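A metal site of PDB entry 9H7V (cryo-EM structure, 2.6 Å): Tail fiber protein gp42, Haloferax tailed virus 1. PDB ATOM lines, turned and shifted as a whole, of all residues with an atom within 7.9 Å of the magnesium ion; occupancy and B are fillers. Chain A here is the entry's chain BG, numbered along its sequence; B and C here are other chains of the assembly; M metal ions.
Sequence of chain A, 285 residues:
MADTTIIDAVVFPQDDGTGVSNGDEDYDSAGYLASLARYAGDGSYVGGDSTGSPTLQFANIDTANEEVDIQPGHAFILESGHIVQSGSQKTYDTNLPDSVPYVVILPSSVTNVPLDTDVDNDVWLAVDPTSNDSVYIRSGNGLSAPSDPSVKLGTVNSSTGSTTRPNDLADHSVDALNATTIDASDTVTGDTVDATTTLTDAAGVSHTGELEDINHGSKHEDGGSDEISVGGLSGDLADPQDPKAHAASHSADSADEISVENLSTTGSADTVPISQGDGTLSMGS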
ATOM      1  N   ALA A   9     -28.239  33.467  37.638  1.00  0.00           N
ATOM      2  CA  ALA A   9     -27.919  33.613  36.221  1.00  0.00           C
ATOM      3  C   ALA A   9     -28.234  32.317  35.466  1.00  0.00           C
ATOM      4  O   ALA A   9     -28.080  31.238  36.016  1.00  0.00           O
ATOM      5  CB  ALA A   9     -26.463  33.976  36.081  1.00  0.00           C
ATOM      6  N   VAL A  10     -28.673  32.458  34.200  1.00  0.00           N
ATOM      7  CA  VAL A  10     -28.976  31.309  33.359  1.00  0.00           C
ATOM      8  C   VAL A  10     -28.256  31.422  32.009  1.00  0.00           C
ATOM      9  O   VAL A  10     -28.160  32.509  31.435  1.00  0.00           O
ATOM     10  CB  VAL A  10     -30.488  31.056  33.195  1.00  0.00           C
ATOM     11  CG1 VAL A  10     -31.136  30.548  34.481  1.00  0.00           C
ATOM     12  CG2 VAL A  10     -31.255  32.255  32.655  1.00  0.00           C
ATOM     13  N   VAL A  11     -27.775  30.265  31.522  1.00  0.00           N
ATOM     14  CA  VAL A  11     -27.016  30.118  30.291  1.00  0.00           C
ATOM     15  C   VAL A  11     -27.773  29.159  29.377  1.00  0.00           C
ATOM     16  O   VAL A  11     -28.219  28.103  29.815  1.00  0.00           O
ATOM     17  CB  VAL A  11     -25.589  29.588  30.570  1.00  0.00           C
ATOM     18  CG1 VAL A  11     -24.780  29.384  29.293  1.00  0.00           C
ATOM     19  CG2 VAL A  11     -24.823  30.474  31.528  1.00  0.00           C
ATOM     20  N   PHE A  12     -27.913  29.544  28.092  1.00  0.00           N
ATOM     21  CA  PHE A  12     -28.611  28.767  27.087  1.00  0.00           C
ATOM     22  C   PHE A  12     -27.999  29.057  25.721  1.00  0.00           C
ATOM     23  O   PHE A  12     -27.572  30.181  25.495  1.00  0.00           O
ATOM     24  CB  PHE A  12     -30.096  29.137  27.090  1.00  0.00           C
ATOM     25  CG  PHE A  12     -30.952  28.373  26.113  1.00  0.00           C
ATOM     26  CD1 PHE A  12     -31.453  27.120  26.456  1.00  0.00           C
ATOM     27  CD2 PHE A  12     -31.245  28.888  24.861  1.00  0.00           C
ATOM     28  CE1 PHE A  12     -32.230  26.404  25.557  1.00  0.00           C
ATOM     29  CE2 PHE A  12     -32.029  28.175  23.968  1.00  0.00           C
ATOM     30  CZ  PHE A  12     -32.524  26.929  24.314  1.00  0.00           C
ATOM     31  N   PRO A  13     -27.941  28.113  24.739  1.00  0.00           N
ATOM     32  CA  PRO A  13     -28.248  26.689  24.935  1.00  0.00           C
ATOM     33  C   PRO A  13     -27.035  25.812  25.273  1.00  0.00           C
ATOM     34  O   PRO A  13     -25.907  26.181  24.935  1.00  0.00           O
ATOM     35  CB  PRO A  13     -28.832  26.337  23.562  1.00  0.00           C
ATOM     36  CG  PRO A  13     -28.036  27.176  22.578  1.00  0.00           C
ATOM     37  CD  PRO A  13     -27.636  28.419  23.331  1.00  0.00           C
ATOM     38  N   GLN A  14     -27.263  24.653  25.915  1.00  0.00           N
ATOM     39  CA  GLN A  14     -26.190  23.789  26.386  1.00  0.00           C
ATOM     40  C   GLN A  14     -26.520  22.302  26.166  1.00  0.00           C
ATOM     41  O   GLN A  14     -27.612  21.856  26.516  1.00  0.00           O
ATOM     42  CB  GLN A  14     -25.849  24.083  27.864  1.00  0.00           C
ATOM     43  CG  GLN A  14     -25.334  25.486  28.122  1.00  0.00           C
ATOM     44  CD  GLN A  14     -25.080  25.786  29.588  1.00  0.00           C
ATOM     45  OE1 GLN A  14     -26.001  25.955  30.373  1.00  0.00           O
ATOM     46  NE2 GLN A  14     -23.809  25.862  29.947  1.00  0.00           N
ATOM     47  N   ASP A  15     -25.551  21.563  25.600  1.00  0.00           N
ATOM     48  CA  ASP A  15     -25.620  20.158  25.202  1.00  0.00           C
ATOM     49  C   ASP A  15     -24.365  19.410  25.650  1.00  0.00           C
ATOM     50  O   ASP A  15     -23.390  20.042  26.052  1.00  0.00           O
ATOM     51  CB  ASP A  15     -25.449  20.006  23.685  1.00  0.00           C
ATOM     52  CG  ASP A  15     -26.549  20.503  22.779  1.00  0.00           C
ATOM     53  OD1 ASP A  15     -27.653  20.831  23.279  1.00  0.00           O
ATOM     54  OD2 ASP A  15     -26.306  20.547  21.563  1.00  0.00           O
ATOM     55  N   VAL A  20     -20.880  20.449  28.715  1.00  0.00           N
ATOM     56  CA  VAL A  20     -21.633  19.887  29.844  1.00  0.00           C
ATOM     57  C   VAL A  20     -21.720  18.369  29.709  1.00  0.00           C
ATOM     58  O   VAL A  20     -21.586  17.832  28.604  1.00  0.00           O
ATOM     59  CB  VAL A  20     -23.030  20.517  30.055  1.00  0.00           C
ATOM     60  CG1 VAL A  20     -23.005  21.950  30.569  1.00  0.00           C
ATOM     61  CG2 VAL A  20     -23.991  20.368  28.885  1.00  0.00           C
ATOM     62  N   ASP A  24     -26.948  16.893  31.993  1.00  0.00           N
ATOM     63  CA  ASP A  24     -26.917  18.304  32.357  1.00  0.00           C
ATOM     64  C   ASP A  24     -27.410  19.225  31.236  1.00  0.00           C
ATOM     65  O   ASP A  24     -27.318  20.442  31.382  1.00  0.00           O
ATOM     66  CB  ASP A  24     -25.507  18.721  32.802  1.00  0.00           C
ATOM     67  CG  ASP A  24     -24.927  17.920  33.961  1.00  0.00           C
ATOM     68  OD1 ASP A  24     -25.718  17.411  34.785  1.00  0.00           O
ATOM     69  OD2 ASP A  24     -23.685  17.830  34.026  1.00  0.00           O
ATOM     70  N   GLU A  25     -27.926  18.664  30.128  1.00  0.00           N
ATOM     71  CA  GLU A  25     -28.346  19.446  28.977  1.00  0.00           C
ATOM     72  C   GLU A  25     -29.535  20.345  29.362  1.00  0.00           C
ATOM     73  O   GLU A  25     -30.378  19.935  30.157  1.00  0.00           O
ATOM     74  CB  GLU A  25     -28.649  18.536  27.794  1.00  0.00           C
ATOM     75  CG  GLU A  25     -27.474  17.663  27.382  1.00  0.00           C
ATOM     76  CD  GLU A  25     -27.642  16.797  26.148  1.00  0.00           C
ATOM     77  OE1 GLU A  25     -27.153  17.183  25.068  1.00  0.00           O
ATOM     78  OE2 GLU A  25     -28.231  15.702  26.274  1.00  0.00           O
ATOM     79  N   ASP A  26     -29.573  21.571  28.805  1.00  0.00           N
ATOM     80  CA  ASP A  26     -30.592  22.575  29.105  1.00  0.00           C
ATOM     81  C   ASP A  26     -31.985  22.052  28.729  1.00  0.00           C
ATOM     82  O   ASP A  26     -32.114  21.247  27.817  1.00  0.00           O
ATOM     83  CB  ASP A  26     -30.355  23.860  28.317  1.00  0.00           C
ATOM     84  CG  ASP A  26     -29.394  24.865  28.948  1.00  0.00           C
ATOM     85  OD1 ASP A  26     -29.313  24.923  30.190  1.00  0.00           O
ATOM     86  OD2 ASP A  26     -28.750  25.602  28.170  1.00  0.00           O
ATOM     87  N   TYR A  27     -33.010  22.553  29.434  1.00  0.00           N
ATOM     88  CA  TYR A  27     -34.389  22.304  29.068  1.00  0.00           C
ATOM     89  C   TYR A  27     -34.835  23.319  28.012  1.00  0.00           C
ATOM     90  O   TYR A  27     -34.290  24.421  27.911  1.00  0.00           O
ATOM     91  CB  TYR A  27     -35.307  22.249  30.292  1.00  0.00           C
ATOM     92  CG  TYR A  27     -35.640  20.859  30.774  1.00  0.00           C
ATOM     93  CD1 TYR A  27     -34.770  20.157  31.601  1.00  0.00           C
ATOM     94  CD2 TYR A  27     -36.826  20.245  30.416  1.00  0.00           C
ATOM     95  CE1 TYR A  27     -35.074  18.885  32.049  1.00  0.00           C
ATOM     96  CE2 TYR A  27     -37.152  18.968  30.855  1.00  0.00           C
ATOM     97  CZ  TYR A  27     -36.266  18.284  31.678  1.00  0.00           C
ATOM     98  OH  TYR A  27     -36.560  17.024  32.116  1.00  0.00           O
ATOM     99  N   TYR A  32     -36.360  30.746  26.354  1.00  0.00           N
ATOM    100  CA  TYR A  32     -34.961  30.552  25.995  1.00  0.00           C
ATOM    101  C   TYR A  32     -34.787  30.658  24.481  1.00  0.00           C
ATOM    102  O   TYR A  32     -33.814  31.270  24.022  1.00  0.00           O
ATOM    103  CB  TYR A  32     -34.455  29.203  26.478  1.00  0.00           C
ATOM    104  CG  TYR A  32     -33.969  29.091  27.905  1.00  0.00           C
ATOM    105  CD1 TYR A  32     -33.312  30.132  28.555  1.00  0.00           C
ATOM    106  CD2 TYR A  32     -34.134  27.901  28.590  1.00  0.00           C
ATOM    107  CE1 TYR A  32     -32.866  29.992  29.862  1.00  0.00           C
ATOM    108  CE2 TYR A  32     -33.683  27.745  29.894  1.00  0.00           C
ATOM    109  CZ  TYR A  32     -33.054  28.797  30.538  1.00  0.00           C
ATOM    110  OH  TYR A  32     -32.615  28.646  31.824  1.00  0.00           O
ATOM    111  N   TYR A 102     -24.064  31.814  23.132  1.00  0.00           N
ATOM    112  CA  TYR A 102     -24.900  31.576  24.293  1.00  0.00           C
ATOM    113  C   TYR A 102     -25.654  32.874  24.608  1.00  0.00           C
ATOM    114  O   TYR A 102     -25.196  33.952  24.241  1.00  0.00           O
ATOM    115  CB  TYR A 102     -24.052  31.291  25.537  1.00  0.00           C
ATOM    116  CG  TYR A 102     -23.218  30.040  25.585  1.00  0.00           C
ATOM    117  CD1 TYR A 102     -23.789  28.778  25.609  1.00  0.00           C
ATOM    118  CD2 TYR A 102     -21.836  30.124  25.713  1.00  0.00           C
ATOM    119  CE1 TYR A 102     -23.006  27.627  25.699  1.00  0.00           C
ATOM    120  CE2 TYR A 102     -21.035  28.994  25.814  1.00  0.00           C
ATOM    121  CZ  TYR A 102     -21.631  27.743  25.803  1.00  0.00           C
ATOM    122  OH  TYR A 102     -20.869  26.610  25.891  1.00  0.00           O
ATOM    123  N   VAL A 103     -26.802  32.751  25.291  1.00  0.00           N
ATOM    124  CA  VAL A 103     -27.413  33.874  25.980  1.00  0.00           C
ATOM    125  C   VAL A 103     -27.143  33.710  27.462  1.00  0.00           C
ATOM    126  O   VAL A 103     -27.374  32.637  28.027  1.00  0.00           O
ATOM    127  CB  VAL A 103     -28.935  34.007  25.729  1.00  0.00           C
ATOM    128  CG1 VAL A 103     -29.450  35.387  26.106  1.00  0.00           C
ATOM    129  CG2 VAL A 103     -29.307  33.691  24.288  1.00  0.00           C
ATOM    130  N   VAL A 127     -18.629  32.557  31.512  1.00  0.00           N
ATOM    131  CA  VAL A 127     -19.382  31.324  31.647  1.00  0.00           C
ATOM    132  C   VAL A 127     -18.380  30.193  31.868  1.00  0.00           C
ATOM    133  O   VAL A 127     -17.294  30.221  31.299  1.00  0.00           O
ATOM    134  CB  VAL A 127     -20.240  31.076  30.383  1.00  0.00           C
ATOM    135  CG1 VAL A 127     -20.973  29.733  30.409  1.00  0.00           C
ATOM    136  CG2 VAL A 127     -21.238  32.210  30.149  1.00  0.00           C
ATOM    137  N   SER A 131     -20.447  22.939  33.494  1.00  0.00           N
ATOM    138  CA  SER A 131     -21.657  22.731  34.272  1.00  0.00           C
ATOM    139  C   SER A 131     -22.718  23.734  33.835  1.00  0.00           C
ATOM    140  O   SER A 131     -22.393  24.789  33.296  1.00  0.00           O
ATOM    141  CB  SER A 131     -21.362  22.827  35.749  1.00  0.00           C
ATOM    142  OG  SER A 131     -22.509  22.494  36.513  1.00  0.00           O
ATOM    143  N   ASN A 132     -23.998  23.395  34.085  1.00  0.00           N
ATOM    144  CA  ASN A 132     -25.119  24.164  33.579  1.00  0.00           C
ATOM    145  C   ASN A 132     -25.319  25.429  34.404  1.00  0.00           C
ATOM    146  O   ASN A 132     -25.387  25.363  35.633  1.00  0.00           O
ATOM    147  CB  ASN A 132     -26.392  23.311  33.488  1.00  0.00           C
ATOM    148  CG  ASN A 132     -27.427  23.856  32.525  1.00  0.00           C
ATOM    149  OD1 ASN A 132     -27.714  25.045  32.508  1.00  0.00           O
ATOM    150  ND2 ASN A 132     -28.010  22.974  31.728  1.00  0.00           N
ATOM    151  N   ASP A 133     -25.369  26.583  33.716  1.00  0.00           N
ATOM    152  CA  ASP A 133     -25.789  27.882  34.232  1.00  0.00           C
ATOM    153  C   ASP A 133     -24.812  28.486  35.249  1.00  0.00           C
ATOM    154  O   ASP A 133     -25.180  29.417  35.965  1.00  0.00           O
ATOM    155  CB  ASP A 133     -27.245  27.867  34.729  1.00  0.00           C
ATOM    156  CG  ASP A 133     -28.297  27.741  33.651  1.00  0.00           C
ATOM    157  OD1 ASP A 133     -27.934  27.733  32.460  1.00  0.00           O
ATOM    158  OD2 ASP A 133     -29.495  27.654  34.005  1.00  0.00           O
ATOM    159  N   SER A 134     -23.572  27.995  35.294  1.00  0.00           N
ATOM    160  CA  SER A 134     -22.556  28.594  36.161  1.00  0.00           C
ATOM    161  C   SER A 134     -21.924  29.813  35.483  1.00  0.00           C
ATOM    162  O   SER A 134     -21.236  29.671  34.476  1.00  0.00           O
ATOM    163  CB  SER A 134     -21.534  27.581  36.622  1.00  0.00           C
ATOM    164  OG  SER A 134     -21.137  26.734  35.554  1.00  0.00           O
ATOM    165  N   GLN B  85     -36.827  27.653  32.612  1.00  0.00           N
ATOM    166  CA  GLN B  85     -36.361  26.571  33.456  1.00  0.00           C
ATOM    167  C   GLN B  85     -34.861  26.719  33.702  1.00  0.00           C
ATOM    168  O   GLN B  85     -34.086  26.700  32.750  1.00  0.00           O
ATOM    169  CB  GLN B  85     -36.669  25.226  32.782  1.00  0.00           C
ATOM    170  CG  GLN B  85     -38.164  24.927  32.627  1.00  0.00           C
ATOM    171  CD  GLN B  85     -38.497  24.077  31.428  1.00  0.00           C
ATOM    172  OE1 GLN B  85     -38.252  24.441  30.286  1.00  0.00           O
ATOM    173  NE2 GLN B  85     -39.099  22.925  31.681  1.00  0.00           N
ATOM    174  N   SER B  86     -34.471  26.862  34.977  1.00  0.00           N
ATOM    175  CA  SER B  86     -33.069  26.943  35.365  1.00  0.00           C
ATOM    176  C   SER B  86     -32.395  25.580  35.214  1.00  0.00           C
ATOM    177  O   SER B  86     -33.011  24.560  35.522  1.00  0.00           O
ATOM    178  CB  SER B  86     -32.927  27.457  36.777  1.00  0.00           C
ATOM    179  OG  SER B  86     -31.574  27.450  37.194  1.00  0.00           O
ATOM    180  N   GLY B  87     -31.148  25.589  34.723  1.00  0.00           N
ATOM    181  CA  GLY B  87     -30.289  24.424  34.680  1.00  0.00           C
ATOM    182  C   GLY B  87     -30.898  23.242  33.937  1.00  0.00           C
ATOM    183  O   GLY B  87     -31.414  23.397  32.835  1.00  0.00           O
ATOM    184  N   SER B  88     -30.834  22.065  34.570  1.00  0.00           N
ATOM    185  CA  SER B  88     -31.389  20.826  34.037  1.00  0.00           C
ATOM    186  C   SER B  88     -32.700  20.478  34.736  1.00  0.00           C
ATOM    187  O   SER B  88     -33.099  19.312  34.766  1.00  0.00           O
ATOM    188  CB  SER B  88     -30.372  19.699  34.125  1.00  0.00           C
ATOM    189  OG  SER B  88     -29.961  19.500  35.466  1.00  0.00           O
ATOM    190  N   LEU C   4     -32.351  19.412  25.552  1.00  0.00           N
ATOM    191  CA  LEU C   4     -31.735  19.516  24.244  1.00  0.00           C
ATOM    192  C   LEU C   4     -30.980  18.222  23.946  1.00  0.00           C
ATOM    193  O   LEU C   4     -30.429  17.613  24.865  1.00  0.00           O
ATOM    194  CB  LEU C   4     -30.774  20.712  24.205  1.00  0.00           C
ATOM    195  CG  LEU C   4     -31.358  22.092  24.529  1.00  0.00           C
ATOM    196  CD1 LEU C   4     -30.303  23.161  24.331  1.00  0.00           C
ATOM    197  CD2 LEU C   4     -32.593  22.403  23.704  1.00  0.00           C
HETATM  198 MG    MG M   1     -27.971  26.374  30.947  1.00  0.00          MG
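Five residues have an atom within 4 Å of the magnesium ion: Val 11, Gln 14, Asp 26, Asn 132 and Asp 133.
The nearest printed residue that does not touch the magnesium ion is Phe 12 (4.3 Å).
The magnesium ion is bound by the side-chain carboxylate of Asp 133, the side-chain amide oxygen of Asn 132, the backbone carbonyl oxygen of Val 11, the side-chain amide oxygen of Gln 14 and the side-chain carboxylate of Asp 26.
The backbone NH of Gly 87 of chain B sits at hydrogen-bond distance from the side-chain carboxylate of Asp 133, at 2.7 Å.
O of Asp 24 sits at hydrogen-bond distance from ND2 of Asn 132, at 2.6 Å.
N of Leu 4 of chain C sits at hydrogen-bond distance from O of Asp 26, at 2.9 Å.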
